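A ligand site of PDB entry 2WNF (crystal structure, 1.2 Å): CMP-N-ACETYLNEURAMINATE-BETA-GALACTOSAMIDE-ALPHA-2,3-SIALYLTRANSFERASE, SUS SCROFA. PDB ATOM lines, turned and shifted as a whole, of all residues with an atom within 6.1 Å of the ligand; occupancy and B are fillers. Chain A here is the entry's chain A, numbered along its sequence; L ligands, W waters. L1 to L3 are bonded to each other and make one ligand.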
ATOM      1  N   LEU A  62     -22.277 -22.282  34.041  1.00  0.00           N
ATOM      2  CA  LEU A  62     -22.728 -23.446  33.255  1.00  0.00           C
ATOM      3  C   LEU A  62     -22.492 -24.737  33.986  1.00  0.00           C
ATOM      4  O   LEU A  62     -23.410 -25.567  34.046  1.00  0.00           O
ATOM      5  CB  LEU A  62     -22.054 -23.558  31.909  1.00  0.00           C
ATOM      6  CG  LEU A  62     -22.178 -22.321  31.042  1.00  0.00           C
ATOM      7  CD1 LEU A  62     -21.589 -22.585  29.689  1.00  0.00           C
ATOM      8  CD2 LEU A  62     -23.718 -21.900  30.976  1.00  0.00           C
ATOM      9  N   GLN A  63     -21.309 -24.942  34.534  1.00  0.00           N
ATOM     10  CA  GLN A  63     -20.975 -26.188  35.246  1.00  0.00           C
ATOM     11  C   GLN A  63     -20.507 -25.992  36.677  1.00  0.00           C
ATOM     12  O   GLN A  63     -20.266 -26.991  37.375  1.00  0.00           O
ATOM     13  CB  GLN A  63     -19.965 -27.021  34.408  1.00  0.00           C
ATOM     14  CG  GLN A  63     -20.556 -27.335  32.996  1.00  0.00           C
ATOM     15  CD  GLN A  63     -19.837 -28.381  32.227  1.00  0.00           C
ATOM     16  OE1 GLN A  63     -18.698 -28.695  32.499  1.00  0.00           O
ATOM     17  NE2 GLN A  63     -20.488 -28.905  31.206  1.00  0.00           N
ATOM     18  N   TYR A 149     -15.215 -32.153  23.663  1.00  0.00           N
ATOM     19  CA  TYR A 149     -14.945 -31.644  25.036  1.00  0.00           C
ATOM     20  C   TYR A 149     -14.353 -32.797  25.811  1.00  0.00           C
ATOM     21  O   TYR A 149     -14.375 -33.936  25.276  1.00  0.00           O
ATOM     22  CB  TYR A 149     -16.201 -30.974  25.636  1.00  0.00           C
ATOM     23  CG  TYR A 149     -17.481 -31.721  25.509  1.00  0.00           C
ATOM     24  CD1 TYR A 149     -18.351 -31.543  24.403  1.00  0.00           C
ATOM     25  CD2 TYR A 149     -17.920 -32.618  26.473  1.00  0.00           C
ATOM     26  CE1 TYR A 149     -19.506 -32.243  24.283  1.00  0.00           C
ATOM     27  CE2 TYR A 149     -19.079 -33.320  26.362  1.00  0.00           C
ATOM     28  CZ  TYR A 149     -19.908 -33.081  25.294  1.00  0.00           C
ATOM     29  OH  TYR A 149     -21.072 -33.828  25.132  1.00  0.00           O
ATOM     30  N   GLU A 151     -15.192 -34.817  28.091  1.00  0.00           N
ATOM     31  CA  GLU A 151     -16.134 -35.879  28.367  1.00  0.00           C
ATOM     32  C   GLU A 151     -16.677 -36.479  27.087  1.00  0.00           C
ATOM     33  O   GLU A 151     -17.497 -37.422  27.170  1.00  0.00           O
ATOM     34  CB  GLU A 151     -17.207 -35.402  29.320  1.00  0.00           C
ATOM     35  CG  GLU A 151     -16.675 -34.767  30.582  1.00  0.00           C
ATOM     36  CD  GLU A 151     -16.294 -33.288  30.509  1.00  0.00           C
ATOM     37  OE1 GLU A 151     -16.361 -32.677  29.383  1.00  0.00           O
ATOM     38  OE2 GLU A 151     -15.915 -32.731  31.557  1.00  0.00           O
ATOM     39  N   PHE A 167     -16.562 -25.653  28.476  1.00  0.00           N
ATOM     40  CA  PHE A 167     -17.730 -25.352  29.281  1.00  0.00           C
ATOM     41  C   PHE A 167     -17.386 -24.978  30.718  1.00  0.00           C
ATOM     42  O   PHE A 167     -18.276 -24.711  31.545  1.00  0.00           O
ATOM     43  CB  PHE A 167     -18.714 -26.575  29.268  1.00  0.00           C
ATOM     44  CG  PHE A 167     -19.273 -26.824  27.892  1.00  0.00           C
ATOM     45  CD1 PHE A 167     -20.343 -26.074  27.430  1.00  0.00           C
ATOM     46  CD2 PHE A 167     -18.705 -27.825  27.086  1.00  0.00           C
ATOM     47  CE1 PHE A 167     -20.856 -26.355  26.112  1.00  0.00           C
ATOM     48  CE2 PHE A 167     -19.207 -28.041  25.794  1.00  0.00           C
ATOM     49  CZ  PHE A 167     -20.249 -27.328  25.368  1.00  0.00           C
ATOM     50  N   LYS A 168     -16.101 -25.045  31.023  1.00  0.00           N
ATOM     51  CA  LYS A 168     -15.560 -24.732  32.375  1.00  0.00           C
ATOM     52  C   LYS A 168     -14.055 -24.529  32.247  1.00  0.00           C
ATOM     53  O   LYS A 168     -13.470 -24.977  31.262  1.00  0.00           O
ATOM     54  CB  LYS A 168     -15.928 -25.807  33.422  1.00  0.00           C
ATOM     55  CG  LYS A 168     -15.382 -27.212  33.023  1.00  0.00           C
ATOM     56  CD  LYS A 168     -15.897 -28.316  34.014  1.00  0.00           C
ATOM     57  CE  LYS A 168     -15.627 -29.698  33.568  1.00  0.00           C
ATOM     58  NZ  LYS A 168     -16.152 -30.044  32.225  1.00  0.00           N
ATOM     59  N   ASP A 171     -11.816 -27.440  31.387  1.00  0.00           N
ATOM     60  CA  ASP A 171     -11.742 -27.968  30.003  1.00  0.00           C
ATOM     61  C   ASP A 171     -10.480 -27.422  29.296  1.00  0.00           C
ATOM     62  O   ASP A 171      -9.871 -28.099  28.460  1.00  0.00           O
ATOM     63  CB  ASP A 171     -12.980 -27.617  29.209  1.00  0.00           C
ATOM     64  CG  ASP A 171     -14.209 -28.353  29.710  1.00  0.00           C
ATOM     65  OD1 ASP A 171     -14.103 -29.266  30.588  1.00  0.00           O
ATOM     66  OD2 ASP A 171     -15.333 -28.042  29.213  1.00  0.00           O
ATOM     67  N   TYR A 188     -16.472 -34.316  35.898  1.00  0.00           N
ATOM     68  CA  TYR A 188     -17.669 -34.886  36.513  1.00  0.00           C
ATOM     69  C   TYR A 188     -17.828 -36.366  36.164  1.00  0.00           C
ATOM     70  O   TYR A 188     -18.637 -37.061  36.791  1.00  0.00           O
ATOM     71  CB  TYR A 188     -18.917 -34.059  36.138  1.00  0.00           C
ATOM     72  CG  TYR A 188     -19.184 -33.882  34.655  1.00  0.00           C
ATOM     73  CD1 TYR A 188     -19.875 -34.840  33.919  1.00  0.00           C
ATOM     74  CD2 TYR A 188     -18.738 -32.716  33.997  1.00  0.00           C
ATOM     75  CE1 TYR A 188     -20.157 -34.637  32.587  1.00  0.00           C
ATOM     76  CE2 TYR A 188     -19.036 -32.495  32.639  1.00  0.00           C
ATOM     77  CZ  TYR A 188     -19.718 -33.482  31.934  1.00  0.00           C
ATOM     78  OH  TYR A 188     -20.032 -33.338  30.579  1.00  0.00           O
ATOM     79  N   VAL A 189     -17.056 -36.833  35.184  1.00  0.00           N
ATOM     80  CA  VAL A 189     -16.931 -38.232  34.801  1.00  0.00           C
ATOM     81  C   VAL A 189     -15.439 -38.464  34.452  1.00  0.00           C
ATOM     82  O   VAL A 189     -14.709 -37.518  34.256  1.00  0.00           O
ATOM     83  CB  VAL A 189     -17.782 -38.635  33.616  1.00  0.00           C
ATOM     84  CG1 VAL A 189     -19.304 -38.683  33.992  1.00  0.00           C
ATOM     85  CG2 VAL A 189     -17.495 -37.703  32.393  1.00  0.00           C
ATOM     86  N   ARG A 223     -30.371 -24.680  29.502  1.00  0.00           N
ATOM     87  CA  ARG A 223     -29.363 -24.186  30.456  1.00  0.00           C
ATOM     88  C   ARG A 223     -28.173 -23.566  29.691  1.00  0.00           C
ATOM     89  O   ARG A 223     -27.611 -22.524  29.998  1.00  0.00           O
ATOM     90  CB  ARG A 223     -28.868 -25.359  31.316  1.00  0.00           C
ATOM     91  CG  ARG A 223     -27.936 -24.983  32.428  1.00  0.00           C
ATOM     92  CD  ARG A 223     -27.579 -26.222  33.258  1.00  0.00           C
ATOM     93  NE  ARG A 223     -28.777 -26.853  33.854  1.00  0.00           N
ATOM     94  CZ  ARG A 223     -28.727 -27.914  34.647  1.00  0.00           C
ATOM     95  NH1 ARG A 223     -27.520 -28.483  34.897  1.00  0.00           N
ATOM     96  NH2 ARG A 223     -29.870 -28.393  35.201  1.00  0.00           N
ATOM     97  N   TYR A 224     -27.807 -24.179  28.526  1.00  0.00           N
ATOM     98  CA  TYR A 224     -26.818 -23.651  27.635  1.00  0.00           C
ATOM     99  C   TYR A 224     -26.952 -24.463  26.316  1.00  0.00           C
ATOM    100  O   TYR A 224     -27.619 -25.450  26.263  1.00  0.00           O
ATOM    101  CB  TYR A 224     -25.399 -23.678  28.225  1.00  0.00           C
ATOM    102  CG  TYR A 224     -24.890 -25.038  28.665  1.00  0.00           C
ATOM    103  CD1 TYR A 224     -24.188 -25.848  27.775  1.00  0.00           C
ATOM    104  CD2 TYR A 224     -25.099 -25.501  29.966  1.00  0.00           C
ATOM    105  CE1 TYR A 224     -23.722 -27.077  28.188  1.00  0.00           C
ATOM    106  CE2 TYR A 224     -24.560 -26.683  30.372  1.00  0.00           C
ATOM    107  CZ  TYR A 224     -23.910 -27.476  29.485  1.00  0.00           C
ATOM    108  OH  TYR A 224     -23.406 -28.720  29.901  1.00  0.00           O
ATOM    109  N   PRO A 225     -26.251 -24.036  25.231  1.00  0.00           N
ATOM    110  CA  PRO A 225     -26.536 -24.642  23.901  1.00  0.00           C
ATOM    111  C   PRO A 225     -25.940 -26.059  23.788  1.00  0.00           C
ATOM    112  O   PRO A 225     -24.841 -26.347  24.326  1.00  0.00           O
ATOM    113  CB  PRO A 225     -25.772 -23.712  22.955  1.00  0.00           C
ATOM    114  CG  PRO A 225     -25.747 -22.365  23.683  1.00  0.00           C
ATOM    115  CD  PRO A 225     -25.468 -22.774  25.135  1.00  0.00           C
ATOM    116  N   SER A 226     -26.601 -26.923  23.027  1.00  0.00           N
ATOM    117  CA  SER A 226     -26.053 -28.253  22.664  1.00  0.00           C
ATOM    118  C   SER A 226     -24.857 -28.065  21.734  1.00  0.00           C
ATOM    119  O   SER A 226     -24.659 -27.020  21.045  1.00  0.00           O
ATOM    120  CB  SER A 226     -27.079 -29.093  21.917  1.00  0.00           C
ATOM    121  OG  SER A 226     -27.274 -28.643  20.587  1.00  0.00           O
ATOM    122  N   THR A 227     -24.051 -29.092  21.671  1.00  0.00           N
ATOM    123  CA  THR A 227     -22.893 -29.085  20.759  1.00  0.00           C
ATOM    124  C   THR A 227     -23.379 -28.977  19.309  1.00  0.00           C
ATOM    125  O   THR A 227     -22.711 -28.311  18.501  1.00  0.00           O
ATOM    126  CB  THR A 227     -22.067 -30.334  21.006  1.00  0.00           C
ATOM    127  OG1 THR A 227     -21.693 -30.310  22.430  1.00  0.00           O
ATOM    128  CG2 THR A 227     -20.734 -30.333  20.155  1.00  0.00           C
ATOM    129  N   GLY A 272     -32.321 -33.135  29.510  1.00  0.00           N
ATOM    130  CA  GLY A 272     -32.558 -32.023  30.430  1.00  0.00           C
ATOM    131  C   GLY A 272     -31.491 -30.950  30.703  1.00  0.00           C
ATOM    132  O   GLY A 272     -31.469 -30.402  31.829  1.00  0.00           O
ATOM    133  N   VAL A 273     -30.613 -30.664  29.718  1.00  0.00           N
ATOM    134  CA  VAL A 273     -29.641 -29.554  29.737  1.00  0.00           C
ATOM    135  C   VAL A 273     -29.881 -28.472  28.570  1.00  0.00           C
ATOM    136  O   VAL A 273     -29.519 -27.281  28.652  1.00  0.00           O
ATOM    137  CB  VAL A 273     -28.153 -30.147  29.494  1.00  0.00           C
ATOM    138  CG1 VAL A 273     -27.145 -29.101  29.695  1.00  0.00           C
ATOM    139  CG2 VAL A 273     -27.902 -31.324  30.488  1.00  0.00           C
ATOM    140  N   HIS A 274     -30.290 -29.060  27.462  1.00  0.00           N
ATOM    141  CA  HIS A 274     -30.517 -28.267  26.212  1.00  0.00           C
ATOM    142  C   HIS A 274     -32.048 -28.287  25.922  1.00  0.00           C
ATOM    143  O   HIS A 274     -32.719 -29.237  26.283  1.00  0.00           O
ATOM    144  CB  HIS A 274     -29.726 -28.858  25.064  1.00  0.00           C
ATOM    145  CG  HIS A 274     -28.329 -29.178  25.460  1.00  0.00           C
ATOM    146  ND1 HIS A 274     -27.470 -28.220  25.977  1.00  0.00           N
ATOM    147  CD2 HIS A 274     -27.672 -30.363  25.472  1.00  0.00           C
ATOM    148  CE1 HIS A 274     -26.317 -28.831  26.257  1.00  0.00           C
ATOM    149  NE2 HIS A 274     -26.392 -30.098  25.934  1.00  0.00           N
HETATM  150  C1  LIG L   1     -23.470 -32.305  29.537  1.00  0.00           C
HETATM  151  C2  LIG L   1     -24.406 -32.169  28.396  1.00  0.00           C
HETATM  152  C3  LIG L   1     -23.715 -32.359  27.058  1.00  0.00           C
HETATM  153  C4  LIG L   1     -22.567 -31.310  26.982  1.00  0.00           C
HETATM  154  C5  LIG L   1     -21.651 -31.530  28.168  1.00  0.00           C
HETATM  155  C6  LIG L   1     -20.488 -30.586  28.205  1.00  0.00           C
HETATM  156  O1  LIG L   1     -25.406 -33.245  28.547  1.00  0.00           O
HETATM  157  O2  LIG L   1     -24.644 -32.160  25.951  1.00  0.00           O
HETATM  158  O3  LIG L   1     -23.137 -29.956  27.065  1.00  0.00           O
HETATM  159  O4  LIG L   1     -22.448 -31.315  29.405  1.00  0.00           O
HETATM  160  O5  LIG L   1     -19.628 -30.949  29.343  1.00  0.00           O
HETATM  161  O1  LG2 L   2     -23.493 -31.983  34.749  1.00  0.00           O
HETATM  162  C1  LG2 L   2     -24.259 -33.083  34.268  1.00  0.00           C
HETATM  163  C2  LG2 L   2     -24.766 -32.699  32.835  1.00  0.00           C
HETATM  164  N1  LG2 L   2     -25.521 -33.835  32.302  1.00  0.00           N
HETATM  165  C3  LG2 L   2     -23.588 -32.362  31.897  1.00  0.00           C
HETATM  166  O2  LG2 L   2     -24.195 -31.927  30.697  1.00  0.00           O
HETATM  167  C4  LG2 L   2     -22.720 -31.295  32.544  1.00  0.00           C
HETATM  168  O3  LG2 L   2     -23.401 -30.043  32.530  1.00  0.00           O
HETATM  169  C5  LG2 L   2     -22.281 -31.655  33.974  1.00  0.00           C
HETATM  170  C6  LG2 L   2     -21.629 -30.479  34.666  1.00  0.00           C
HETATM  171  O4  LG2 L   2     -21.029 -31.044  35.903  1.00  0.00           O
HETATM  172  C7  LG2 L   2     -26.851 -33.924  32.458  1.00  0.00           C
HETATM  173  O5  LG2 L   2     -27.452 -33.143  33.215  1.00  0.00           O
HETATM  174  C8  LG2 L   2     -27.447 -35.202  31.867  1.00  0.00           C
HETATM  175  N1  LG3 L   3     -23.044 -36.931  33.625  1.00  0.00           N
HETATM  176  O1  LG3 L   3     -24.312 -36.720  33.027  1.00  0.00           O
HETATM  177  O2  LG3 L   3     -22.336 -38.041  33.073  1.00  0.00           O
HETATM  178  C1  LG3 L   3     -22.834 -36.410  34.846  1.00  0.00           C
HETATM  179  C2  LG3 L   3     -23.087 -35.085  35.155  1.00  0.00           C
HETATM  180  C3  LG3 L   3     -22.920 -34.522  36.391  1.00  0.00           C
HETATM  181  C4  LG3 L   3     -22.466 -35.414  37.444  1.00  0.00           C
HETATM  182  C5  LG3 L   3     -22.248 -36.704  37.083  1.00  0.00           C
HETATM  183  C6  LG3 L   3     -22.420 -37.309  35.867  1.00  0.00           C
HETATM  184  O3  LG3 L   3     -23.501 -34.274  34.073  1.00  0.00           O
HETATM  185  O   HOH W   1     -24.807 -31.586  23.037  1.00  0.00           O
HETATM  186  O   HOH W   2     -27.259 -31.100  34.747  1.00  0.00           O
HETATM  187  O   HOH W   3     -17.155 -30.128  29.322  1.00  0.00           O
HETATM  188  O   HOH W   4     -23.225 -28.674  24.729  1.00  0.00           O
HETATM  189  O   HOH W   5     -24.143 -35.816  30.549  1.00  0.00           O
HETATM  190  O   HOH W   6     -22.870 -30.775  37.941  1.00  0.00           O
HETATM  191  O   HOH W   7     -19.136 -29.480  36.972  1.00  0.00           O
HETATM  192  O   HOH W   8     -24.774 -28.298  34.339  1.00  0.00           O
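An oxygen (O2) of LIG L1 sits at hydrogen-bond distance from a ring nitrogen (NE2) of His 274 (2.7 Å). O5 of LIG L1 lies within hydrogen-bond range of OH of Tyr 188 (2.7 Å). An oxygen (O4) of LIG L1 sits at hydrogen-bond distance from the side-chain hydroxyl of Tyr 224 (2.8 Å). The side-chain amide nitrogen (NE2) of Gln 63 is in hydrogen-bond range of an oxygen (O5) of LIG L1 (2.9 Å).
O of Tyr 224 sits at hydrogen-bond distance from ND1 of His 274 (2.8 Å). A ring nitrogen (ND1) of His 274 is in hydrogen-bond range of the backbone NH (N) of Ser 226. The side-chain hydroxyl (OH) of Tyr 224 lies within hydrogen-bond range of the side-chain amide nitrogen (NE2) of Gln 63 (3.2 Å). The side-chain amino group of Lys 168 is in hydrogen-bond range of the side-chain amide oxygen of Gln 63 (2.9 Å). The backbone NH (N) of Arg 223 lies within hydrogen-bond range of the backbone carbonyl oxygen (O) of Val 273 (2.9 Å). N of Phe 167 sits at hydrogen-bond distance from OD2 of Asp 171, 2.8 Å away. The side-chain carboxylate of Glu 151 lies within salt-bridge range of the side-chain amino group of Lys 168, 2.8 Å away.
Residues that only touch the ligand: Val 189 (3.2 Å), Val 273 (3.3 Å), Tyr 149 (3.5 Å), Phe 167 (3.5 Å) and Glu 151 (3.7 Å). Within 4 Å of the ligand: Gln 63, Tyr 149, Glu 151, Phe 167, Tyr 188, Val 189, Tyr 224, Val 273 and His 274.
Water W2 lies within hydrogen-bond range of O5 of LG2 L2 (2.6 Å) and NH1 of Arg 223 (2.6 Å). Water W3 lies within hydrogen-bond range of an oxygen (O5) of LIG L1 (2.6 Å), the side-chain carboxylate of Glu 151 (2.7 Å), the side-chain carboxylate of Asp 171 (2.8 Å) and the side-chain amino group of Lys 168 (3.1 Å). Water W4 lies within hydrogen-bond range of an oxygen (O3) of LIG L1, the backbone carbonyl oxygen (O) of Pro 225 and the backbone NH (N) of Thr 227. Water W7 lies within hydrogen-bond range of an oxygen (O4) of LG2 L2 (2.7 Å) and the backbone carbonyl oxygen of Gln 63 (2.8 Å). Water W8 lies within hydrogen-bond range of the guanidinium group (NH1) of Arg 223 (2.8 Å), an oxygen (O3) of LG2 L2 (2.9 Å) and the backbone carbonyl oxygen (O) of Leu 62 (3.1 Å). Water W1 bridges the backbone NH of Thr 227 and an oxygen (O2) of LIG L1.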
